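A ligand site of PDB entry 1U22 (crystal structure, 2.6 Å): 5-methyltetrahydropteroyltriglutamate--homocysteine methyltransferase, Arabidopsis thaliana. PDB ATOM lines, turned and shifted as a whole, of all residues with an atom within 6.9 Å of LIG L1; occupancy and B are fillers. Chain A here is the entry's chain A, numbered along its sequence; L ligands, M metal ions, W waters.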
ATOM      1  N   ILE A 437      32.414  20.245 -14.509  1.00  0.00           N
ATOM      2  CA  ILE A 437      31.580  19.648 -13.492  1.00  0.00           C
ATOM      3  C   ILE A 437      30.304  20.410 -13.111  1.00  0.00           C
ATOM      4  O   ILE A 437      29.278  19.783 -12.854  1.00  0.00           O
ATOM      5  CB  ILE A 437      32.397  19.384 -12.229  1.00  0.00           C
ATOM      6  CG1 ILE A 437      33.626  18.544 -12.585  1.00  0.00           C
ATOM      7  CG2 ILE A 437      31.527  18.715 -11.181  1.00  0.00           C
ATOM      8  CD1 ILE A 437      33.323  17.221 -13.263  1.00  0.00           C
ATOM      9  N   GLY A 438      30.368  21.732 -13.072  1.00  0.00           N
ATOM     10  CA  GLY A 438      29.171  22.477 -12.730  1.00  0.00           C
ATOM     11  C   GLY A 438      29.385  23.931 -12.429  1.00  0.00           C
ATOM     12  O   GLY A 438      28.806  24.808 -13.076  1.00  0.00           O
ATOM     13  N   SER A 439      30.226  24.194 -11.438  1.00  0.00           N
ATOM     14  CA  SER A 439      30.531  25.555 -11.008  1.00  0.00           C
ATOM     15  C   SER A 439      31.751  26.151 -11.697  1.00  0.00           C
ATOM     16  O   SER A 439      32.592  25.431 -12.263  1.00  0.00           O
ATOM     17  CB  SER A 439      30.705  25.591  -9.482  1.00  0.00           C
ATOM     18  OG  SER A 439      31.710  24.691  -9.026  1.00  0.00           O
ATOM     19  N   PHE A 440      31.843  27.485 -11.640  1.00  0.00           N
ATOM     20  CA  PHE A 440      32.950  28.217 -12.232  1.00  0.00           C
ATOM     21  C   PHE A 440      33.428  29.345 -11.340  1.00  0.00           C
ATOM     22  O   PHE A 440      32.682  29.835 -10.493  1.00  0.00           O
ATOM     23  CB  PHE A 440      32.561  28.775 -13.591  1.00  0.00           C
ATOM     24  CG  PHE A 440      33.027  27.943 -14.726  1.00  0.00           C
ATOM     25  CD1 PHE A 440      32.439  26.724 -14.993  1.00  0.00           C
ATOM     26  CD2 PHE A 440      34.119  28.350 -15.482  1.00  0.00           C
ATOM     27  CE1 PHE A 440      32.928  25.907 -16.002  1.00  0.00           C
ATOM     28  CE2 PHE A 440      34.614  27.551 -16.491  1.00  0.00           C
ATOM     29  CZ  PHE A 440      34.020  26.314 -16.758  1.00  0.00           C
ATOM     30  N   GLU A 490      26.956  27.647 -12.985  1.00  0.00           N
ATOM     31  CA  GLU A 490      26.110  27.955 -11.811  1.00  0.00           C
ATOM     32  C   GLU A 490      26.234  29.349 -11.192  1.00  0.00           C
ATOM     33  O   GLU A 490      26.272  29.480  -9.952  1.00  0.00           O
ATOM     34  CB  GLU A 490      26.371  26.961 -10.669  1.00  0.00           C
ATOM     35  CG  GLU A 490      25.902  25.544 -10.837  1.00  0.00           C
ATOM     36  CD  GLU A 490      26.500  24.655  -9.757  1.00  0.00           C
ATOM     37  OE1 GLU A 490      26.303  24.952  -8.553  1.00  0.00           O
ATOM     38  OE2 GLU A 490      27.187  23.673 -10.126  1.00  0.00           O
ATOM     39  N   ASN A 494      24.389  30.121  -5.252  1.00  0.00           N
ATOM     40  CA  ASN A 494      25.430  30.222  -4.214  1.00  0.00           C
ATOM     41  C   ASN A 494      25.652  28.788  -3.716  1.00  0.00           C
ATOM     42  O   ASN A 494      26.631  28.128  -4.098  1.00  0.00           O
ATOM     43  CB  ASN A 494      24.966  31.086  -3.036  1.00  0.00           C
ATOM     44  CG  ASN A 494      24.489  32.471  -3.453  1.00  0.00           C
ATOM     45  OD1 ASN A 494      25.212  33.218  -4.123  1.00  0.00           O
ATOM     46  ND2 ASN A 494      23.281  32.830  -3.043  1.00  0.00           N
ATOM     47  N   MET A 496      24.621  25.060  -3.745  1.00  0.00           N
ATOM     48  CA  MET A 496      23.958  24.102  -4.601  1.00  0.00           C
ATOM     49  C   MET A 496      22.793  23.370  -3.938  1.00  0.00           C
ATOM     50  O   MET A 496      21.966  22.788  -4.633  1.00  0.00           O
ATOM     51  CB  MET A 496      24.975  23.099  -5.156  1.00  0.00           C
ATOM     52  CG  MET A 496      25.944  22.579  -4.120  1.00  0.00           C
ATOM     53  SD  MET A 496      26.302  20.707  -4.366  1.00  0.00           S
ATOM     54  CE  MET A 496      25.049  19.993  -3.091  1.00  0.00           C
ATOM     55  N   MET A 557      21.972  21.368 -15.092  1.00  0.00           N
ATOM     56  CA  MET A 557      22.510  21.096 -13.764  1.00  0.00           C
ATOM     57  C   MET A 557      21.496  20.890 -12.676  1.00  0.00           C
ATOM     58  O   MET A 557      20.571  21.686 -12.518  1.00  0.00           O
ATOM     59  CB  MET A 557      23.451  22.227 -13.345  1.00  0.00           C
ATOM     60  CG  MET A 557      24.887  22.065 -13.793  1.00  0.00           C
ATOM     61  SD  MET A 557      25.702  20.559 -12.924  1.00  0.00           S
ATOM     62  CE  MET A 557      25.341  21.069 -11.100  1.00  0.00           C
ATOM     63  N   LEU A 558      21.671  19.825 -11.918  1.00  0.00           N
ATOM     64  CA  LEU A 558      20.764  19.529 -10.818  1.00  0.00           C
ATOM     65  C   LEU A 558      21.533  18.942  -9.644  1.00  0.00           C
ATOM     66  O   LEU A 558      22.662  18.477  -9.805  1.00  0.00           O
ATOM     67  CB  LEU A 558      19.674  18.554 -11.284  1.00  0.00           C
ATOM     68  CG  LEU A 558      18.664  19.046 -12.330  1.00  0.00           C
ATOM     69  CD1 LEU A 558      17.910  17.869 -12.917  1.00  0.00           C
ATOM     70  CD2 LEU A 558      17.708  20.061 -11.697  1.00  0.00           C
ATOM     71  N   THR A 559      20.904  18.985  -8.470  1.00  0.00           N
ATOM     72  CA  THR A 559      21.474  18.436  -7.248  1.00  0.00           C
ATOM     73  C   THR A 559      20.632  17.219  -6.855  1.00  0.00           C
ATOM     74  O   THR A 559      19.438  17.359  -6.568  1.00  0.00           O
ATOM     75  CB  THR A 559      21.450  19.466  -6.087  1.00  0.00           C
ATOM     76  OG1 THR A 559      22.377  20.517  -6.375  1.00  0.00           O
ATOM     77  CG2 THR A 559      21.829  18.804  -4.758  1.00  0.00           C
ATOM     78  N   TRP A 567      22.653  16.935   3.482  1.00  0.00           N
ATOM     79  CA  TRP A 567      23.072  18.276   3.861  1.00  0.00           C
ATOM     80  C   TRP A 567      21.887  19.186   4.142  1.00  0.00           C
ATOM     81  O   TRP A 567      21.658  20.164   3.431  1.00  0.00           O
ATOM     82  CB  TRP A 567      23.929  18.886   2.755  1.00  0.00           C
ATOM     83  CG  TRP A 567      25.209  18.167   2.568  1.00  0.00           C
ATOM     84  CD1 TRP A 567      25.806  17.350   3.464  1.00  0.00           C
ATOM     85  CD2 TRP A 567      26.098  18.289   1.450  1.00  0.00           C
ATOM     86  NE1 TRP A 567      27.031  16.943   2.979  1.00  0.00           N
ATOM     87  CE2 TRP A 567      27.243  17.508   1.749  1.00  0.00           C
ATOM     88  CE3 TRP A 567      26.052  18.976   0.229  1.00  0.00           C
ATOM     89  CZ2 TRP A 567      28.327  17.397   0.871  1.00  0.00           C
ATOM     90  CZ3 TRP A 567      27.145  18.872  -0.658  1.00  0.00           C
ATOM     91  CH2 TRP A 567      28.271  18.087  -0.321  1.00  0.00           C
ATOM     92  N   GLN A 603      23.394  16.568 -16.249  1.00  0.00           N
ATOM     93  CA  GLN A 603      24.149  16.007 -15.130  1.00  0.00           C
ATOM     94  C   GLN A 603      23.487  16.222 -13.761  1.00  0.00           C
ATOM     95  O   GLN A 603      23.251  17.346 -13.318  1.00  0.00           O
ATOM     96  CB  GLN A 603      25.559  16.589 -15.123  1.00  0.00           C
ATOM     97  CG  GLN A 603      26.052  16.978 -13.749  1.00  0.00           C
ATOM     98  CD  GLN A 603      27.474  17.494 -13.767  1.00  0.00           C
ATOM     99  OE1 GLN A 603      27.826  18.387 -14.542  1.00  0.00           O
ATOM    100  NE2 GLN A 603      28.316  16.920 -12.910  1.00  0.00           N
ATOM    101  N   ASP A 605      23.961  15.502  -9.778  1.00  0.00           N
ATOM    102  CA  ASP A 605      25.073  15.174  -8.890  1.00  0.00           C
ATOM    103  C   ASP A 605      24.706  14.760  -7.472  1.00  0.00           C
ATOM    104  O   ASP A 605      23.795  15.305  -6.859  1.00  0.00           O
ATOM    105  CB  ASP A 605      26.097  16.334  -8.874  1.00  0.00           C
ATOM    106  CG  ASP A 605      25.465  17.688  -8.537  1.00  0.00           C
ATOM    107  OD1 ASP A 605      26.156  18.718  -8.688  1.00  0.00           O
ATOM    108  OD2 ASP A 605      24.286  17.709  -8.119  1.00  0.00           O
ATOM    109  N   GLU A 606      25.441  13.763  -6.983  1.00  0.00           N
ATOM    110  CA  GLU A 606      25.258  13.221  -5.650  1.00  0.00           C
ATOM    111  C   GLU A 606      26.593  13.237  -4.894  1.00  0.00           C
ATOM    112  O   GLU A 606      27.270  12.224  -4.721  1.00  0.00           O
ATOM    113  CB  GLU A 606      24.702  11.803  -5.742  1.00  0.00           C
ATOM    114  CG  GLU A 606      23.232  11.786  -6.115  1.00  0.00           C
ATOM    115  CD  GLU A 606      22.352  12.327  -5.001  1.00  0.00           C
ATOM    116  OE1 GLU A 606      22.604  13.442  -4.507  1.00  0.00           O
ATOM    117  OE2 GLU A 606      21.400  11.624  -4.621  1.00  0.00           O
ATOM    118  N   ALA A 607      26.937  14.447  -4.460  1.00  0.00           N
ATOM    119  CA  ALA A 607      28.154  14.684  -3.733  1.00  0.00           C
ATOM    120  C   ALA A 607      28.141  13.956  -2.405  1.00  0.00           C
ATOM    121  O   ALA A 607      29.147  13.351  -2.026  1.00  0.00           O
ATOM    122  CB  ALA A 607      28.327  16.182  -3.510  1.00  0.00           C
ATOM    123  N   HIS A 647      27.125  12.950 -10.736  1.00  0.00           N
ATOM    124  CA  HIS A 647      28.390  13.400 -10.194  1.00  0.00           C
ATOM    125  C   HIS A 647      28.588  13.248  -8.676  1.00  0.00           C
ATOM    126  O   HIS A 647      27.944  13.946  -7.887  1.00  0.00           O
ATOM    127  CB  HIS A 647      28.633  14.855 -10.602  1.00  0.00           C
ATOM    128  CG  HIS A 647      30.024  15.310 -10.312  1.00  0.00           C
ATOM    129  ND1 HIS A 647      31.132  14.730 -10.887  1.00  0.00           N
ATOM    130  CD2 HIS A 647      30.492  16.241  -9.438  1.00  0.00           C
ATOM    131  CE1 HIS A 647      32.219  15.263 -10.369  1.00  0.00           C
ATOM    132  NE2 HIS A 647      31.867  16.179  -9.490  1.00  0.00           N
ATOM    133  N   CYS A 649      31.384  13.009  -5.315  1.00  0.00           N
ATOM    134  CA  CYS A 649      32.715  13.425  -4.868  1.00  0.00           C
ATOM    135  C   CYS A 649      33.451  12.368  -4.061  1.00  0.00           C
ATOM    136  O   CYS A 649      33.701  12.543  -2.869  1.00  0.00           O
ATOM    137  CB  CYS A 649      32.586  14.698  -4.036  1.00  0.00           C
ATOM    138  SG  CYS A 649      31.401  15.868  -4.717  1.00  0.00           S
ATOM    139  N   CYS A 733      36.069  18.270  -9.885  1.00  0.00           N
ATOM    140  CA  CYS A 733      34.832  18.820  -9.344  1.00  0.00           C
ATOM    141  C   CYS A 733      34.711  20.283  -9.791  1.00  0.00           C
ATOM    142  O   CYS A 733      35.625  20.805 -10.428  1.00  0.00           O
ATOM    143  CB  CYS A 733      34.816  18.741  -7.811  1.00  0.00           C
ATOM    144  SG  CYS A 733      33.267  19.317  -7.037  1.00  0.00           S
ATOM    145  N   GLY A 734      33.593  20.916  -9.477  1.00  0.00           N
ATOM    146  CA  GLY A 734      33.385  22.304  -9.864  1.00  0.00           C
ATOM    147  C   GLY A 734      34.622  23.181  -9.720  1.00  0.00           C
ATOM    148  O   GLY A 734      35.441  22.976  -8.812  1.00  0.00           O
ATOM    149  N   LEU A 735      34.758  24.169 -10.599  1.00  0.00           N
ATOM    150  CA  LEU A 735      35.908  25.064 -10.585  1.00  0.00           C
ATOM    151  C   LEU A 735      35.642  26.309  -9.743  1.00  0.00           C
ATOM    152  O   LEU A 735      36.415  27.270  -9.778  1.00  0.00           O
ATOM    153  CB  LEU A 735      36.249  25.497 -12.029  1.00  0.00           C
ATOM    154  CG  LEU A 735      36.538  24.389 -13.041  1.00  0.00           C
ATOM    155  CD1 LEU A 735      36.612  25.021 -14.401  1.00  0.00           C
ATOM    156  CD2 LEU A 735      37.836  23.640 -12.704  1.00  0.00           C
ATOM    157  N   LYS A 736      34.571  26.277  -8.956  1.00  0.00           N
ATOM    158  CA  LYS A 736      34.166  27.412  -8.134  1.00  0.00           C
ATOM    159  C   LYS A 736      35.208  28.028  -7.230  1.00  0.00           C
ATOM    160  O   LYS A 736      35.218  29.244  -7.038  1.00  0.00           O
ATOM    161  CB  LYS A 736      32.944  27.030  -7.288  1.00  0.00           C
ATOM    162  CG  LYS A 736      32.399  28.171  -6.456  1.00  0.00           C
ATOM    163  CD  LYS A 736      31.019  27.871  -5.922  1.00  0.00           C
ATOM    164  CE  LYS A 736      30.388  29.133  -5.360  1.00  0.00           C
ATOM    165  NZ  LYS A 736      28.889  29.047  -5.332  1.00  0.00           N
HETATM  166  N1  LIG L   1      28.832  20.499  -9.772  1.00  0.00           N
HETATM  167  C1  LIG L   1      28.434  21.141  -8.488  1.00  0.00           C
HETATM  168  C2  LIG L   1      28.225  20.075  -7.402  1.00  0.00           C
HETATM  169  C3  LIG L   1      29.474  19.291  -7.003  1.00  0.00           C
HETATM  170  S1  LIG L   1      29.785  19.379  -5.214  1.00  0.00           S
HETATM  171  C4  LIG L   1      29.502  22.144  -8.033  1.00  0.00           C
HETATM  172  O1  LIG L   1      29.317  22.741  -6.949  1.00  0.00           O
HETATM  173  O2  LIG L   1      30.495  22.300  -8.770  1.00  0.00           O
HETATM  174  N1  LG2 L   2      25.922  22.741   0.774  1.00  0.00           N
HETATM  175  C1  LG2 L   2      25.174  22.581   1.915  1.00  0.00           C
HETATM  176  N2  LG2 L   2      25.741  21.957   2.978  1.00  0.00           N
HETATM  177  C2  LG2 L   2      27.040  21.498   2.938  1.00  0.00           C
HETATM  178  C3  LG2 L   2      27.851  21.647   1.782  1.00  0.00           C
HETATM  179  C4  LG2 L   2      27.235  22.298   0.676  1.00  0.00           C
HETATM  180  N3  LG2 L   2      27.601  20.845   4.080  1.00  0.00           N
HETATM  181  C5  LG2 L   2      28.964  20.334   4.137  1.00  0.00           C
HETATM  182  C6  LG2 L   2      29.778  20.492   2.981  1.00  0.00           C
HETATM  183  N4  LG2 L   2      29.207  21.189   1.707  1.00  0.00           N
HETATM  184  C7  LG2 L   2      31.137  19.933   3.238  1.00  0.00           C
HETATM  185  N5  LG2 L   2      31.919  20.684   4.322  1.00  0.00           N
HETATM  186  C8  LG2 L   2      32.255  22.028   4.362  1.00  0.00           C
HETATM  187  C9  LG2 L   2      31.903  22.992   3.352  1.00  0.00           C
HETATM  188  C10 LG2 L   2      32.267  24.360   3.482  1.00  0.00           C
HETATM  189  C11 LG2 L   2      32.995  24.802   4.621  1.00  0.00           C
HETATM  190  C12 LG2 L   2      33.358  23.856   5.623  1.00  0.00           C
HETATM  191  C13 LG2 L   2      32.986  22.480   5.501  1.00  0.00           C
HETATM  192  C14 LG2 L   2      33.377  26.291   4.746  1.00  0.00           C
HETATM  193  N6  LG2 L   2      32.463  27.049   5.401  1.00  0.00           N
HETATM  194  C15 LG2 L   2      32.550  28.513   5.633  1.00  0.00           C
HETATM  195  C16 LG2 L   2      32.788  28.834   7.132  1.00  0.00           C
HETATM  196  O1  LG2 L   2      33.922  29.293   7.413  1.00  0.00           O
HETATM  197  O2  LG2 L   2      31.855  28.627   7.938  1.00  0.00           O
HETATM  198  C17 LG2 L   2      31.302  29.253   5.133  1.00  0.00           C
HETATM  199  C18 LG2 L   2      31.047  28.939   3.658  1.00  0.00           C
HETATM  200  C19 LG2 L   2      29.815  29.652   3.126  1.00  0.00           C
HETATM  201  O3  LG2 L   2      29.950  30.871   2.853  1.00  0.00           O
HETATM  202  O4  LG2 L   2      28.758  28.967   2.985  1.00  0.00           O
HETATM  203  O5  LG2 L   2      34.446  26.720   4.256  1.00  0.00           O
HETATM  204  O6  LG2 L   2      27.938  22.484  -0.479  1.00  0.00           O
HETATM  205  N7  LG2 L   2      23.903  23.020   1.993  1.00  0.00           N
HETATM  206 ZN    ZN M   1      32.585  16.721  -6.784  1.00  0.00          ZN
HETATM  207  O   HOH W   1      27.521  25.202  -6.078  1.00  0.00           O
HETATM  208  O   HOH W   2      27.097  18.434 -11.022  1.00  0.00           O
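N1 of LIG L1 is in salt-bridge range of OE2 of Glu 490 (3.6 Å).
The side-chain carboxylate (OD1) of Asp 605 is in salt-bridge range of a nitrogen (N1) of LIG L1.
N of Ser 439 lies within hydrogen-bond range of O2 of LIG L1, at 3.3 Å.
The side-chain hydroxyl (OG) of Ser 439 is in hydrogen-bond range of an oxygen (O2) of LIG L1, 2.7 Å away.
N of Gly 734 lies close to O2 of LIG L1 (3.5 Å).
N1 of LIG L1 sits at hydrogen-bond distance from O of Ile 437, 3.2 Å away.
O of Leu 558 sits close to N of Asp 605.
The backbone carbonyl oxygen of Ile 437 sits close to the side-chain amide oxygen of Gln 603 (2.6 Å).
The backbone NH of Ser 439 is in hydrogen-bond range of the side-chain carboxylate of Glu 490 (3.4 Å).
The backbone NH (N) of Glu 490 lies within hydrogen-bond range of the backbone carbonyl oxygen (O) of Gly 438 (3.4 Å).
The side-chain hydroxyl (OG) of Ser 439 sits close to the backbone NH (N) of Lys 736.
The backbone carbonyl oxygen (O) of Ser 439 is in hydrogen-bond range of the backbone NH (N) of Leu 735, 3.0 Å away.
O of Met 496 sits at hydrogen-bond distance from OG1 of Thr 559 (2.9 Å).
The side-chain amide oxygen of Gln 603 lies close to the side-chain sulfur of Met 557 (3.4 Å).
Residues that only touch LIG L1: Gly 438, Met 496, Met 557, Ala 607, Cys 649 and Cys 733.
Hydrophobic or aromatic side chains within 4 Å of LIG L1: Ile 437, Met 496, Met 557 and Ala 607.
Within 4 Å of LIG L1: Ile 437, Gly 438, Ser 439, Glu 490, Met 496, Met 557, Asp 605, Ala 607, Cys 649, Cys 733 and Gly 734.
The nearest printed residue that does not touch LIG L1 is His 647 (4.03 Å).
Water W1 lies within hydrogen-bond range of the side-chain carboxylate (OE1) of Glu 490 (2.8 Å) and an oxygen (O1) of LIG L1 (3.2 Å).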
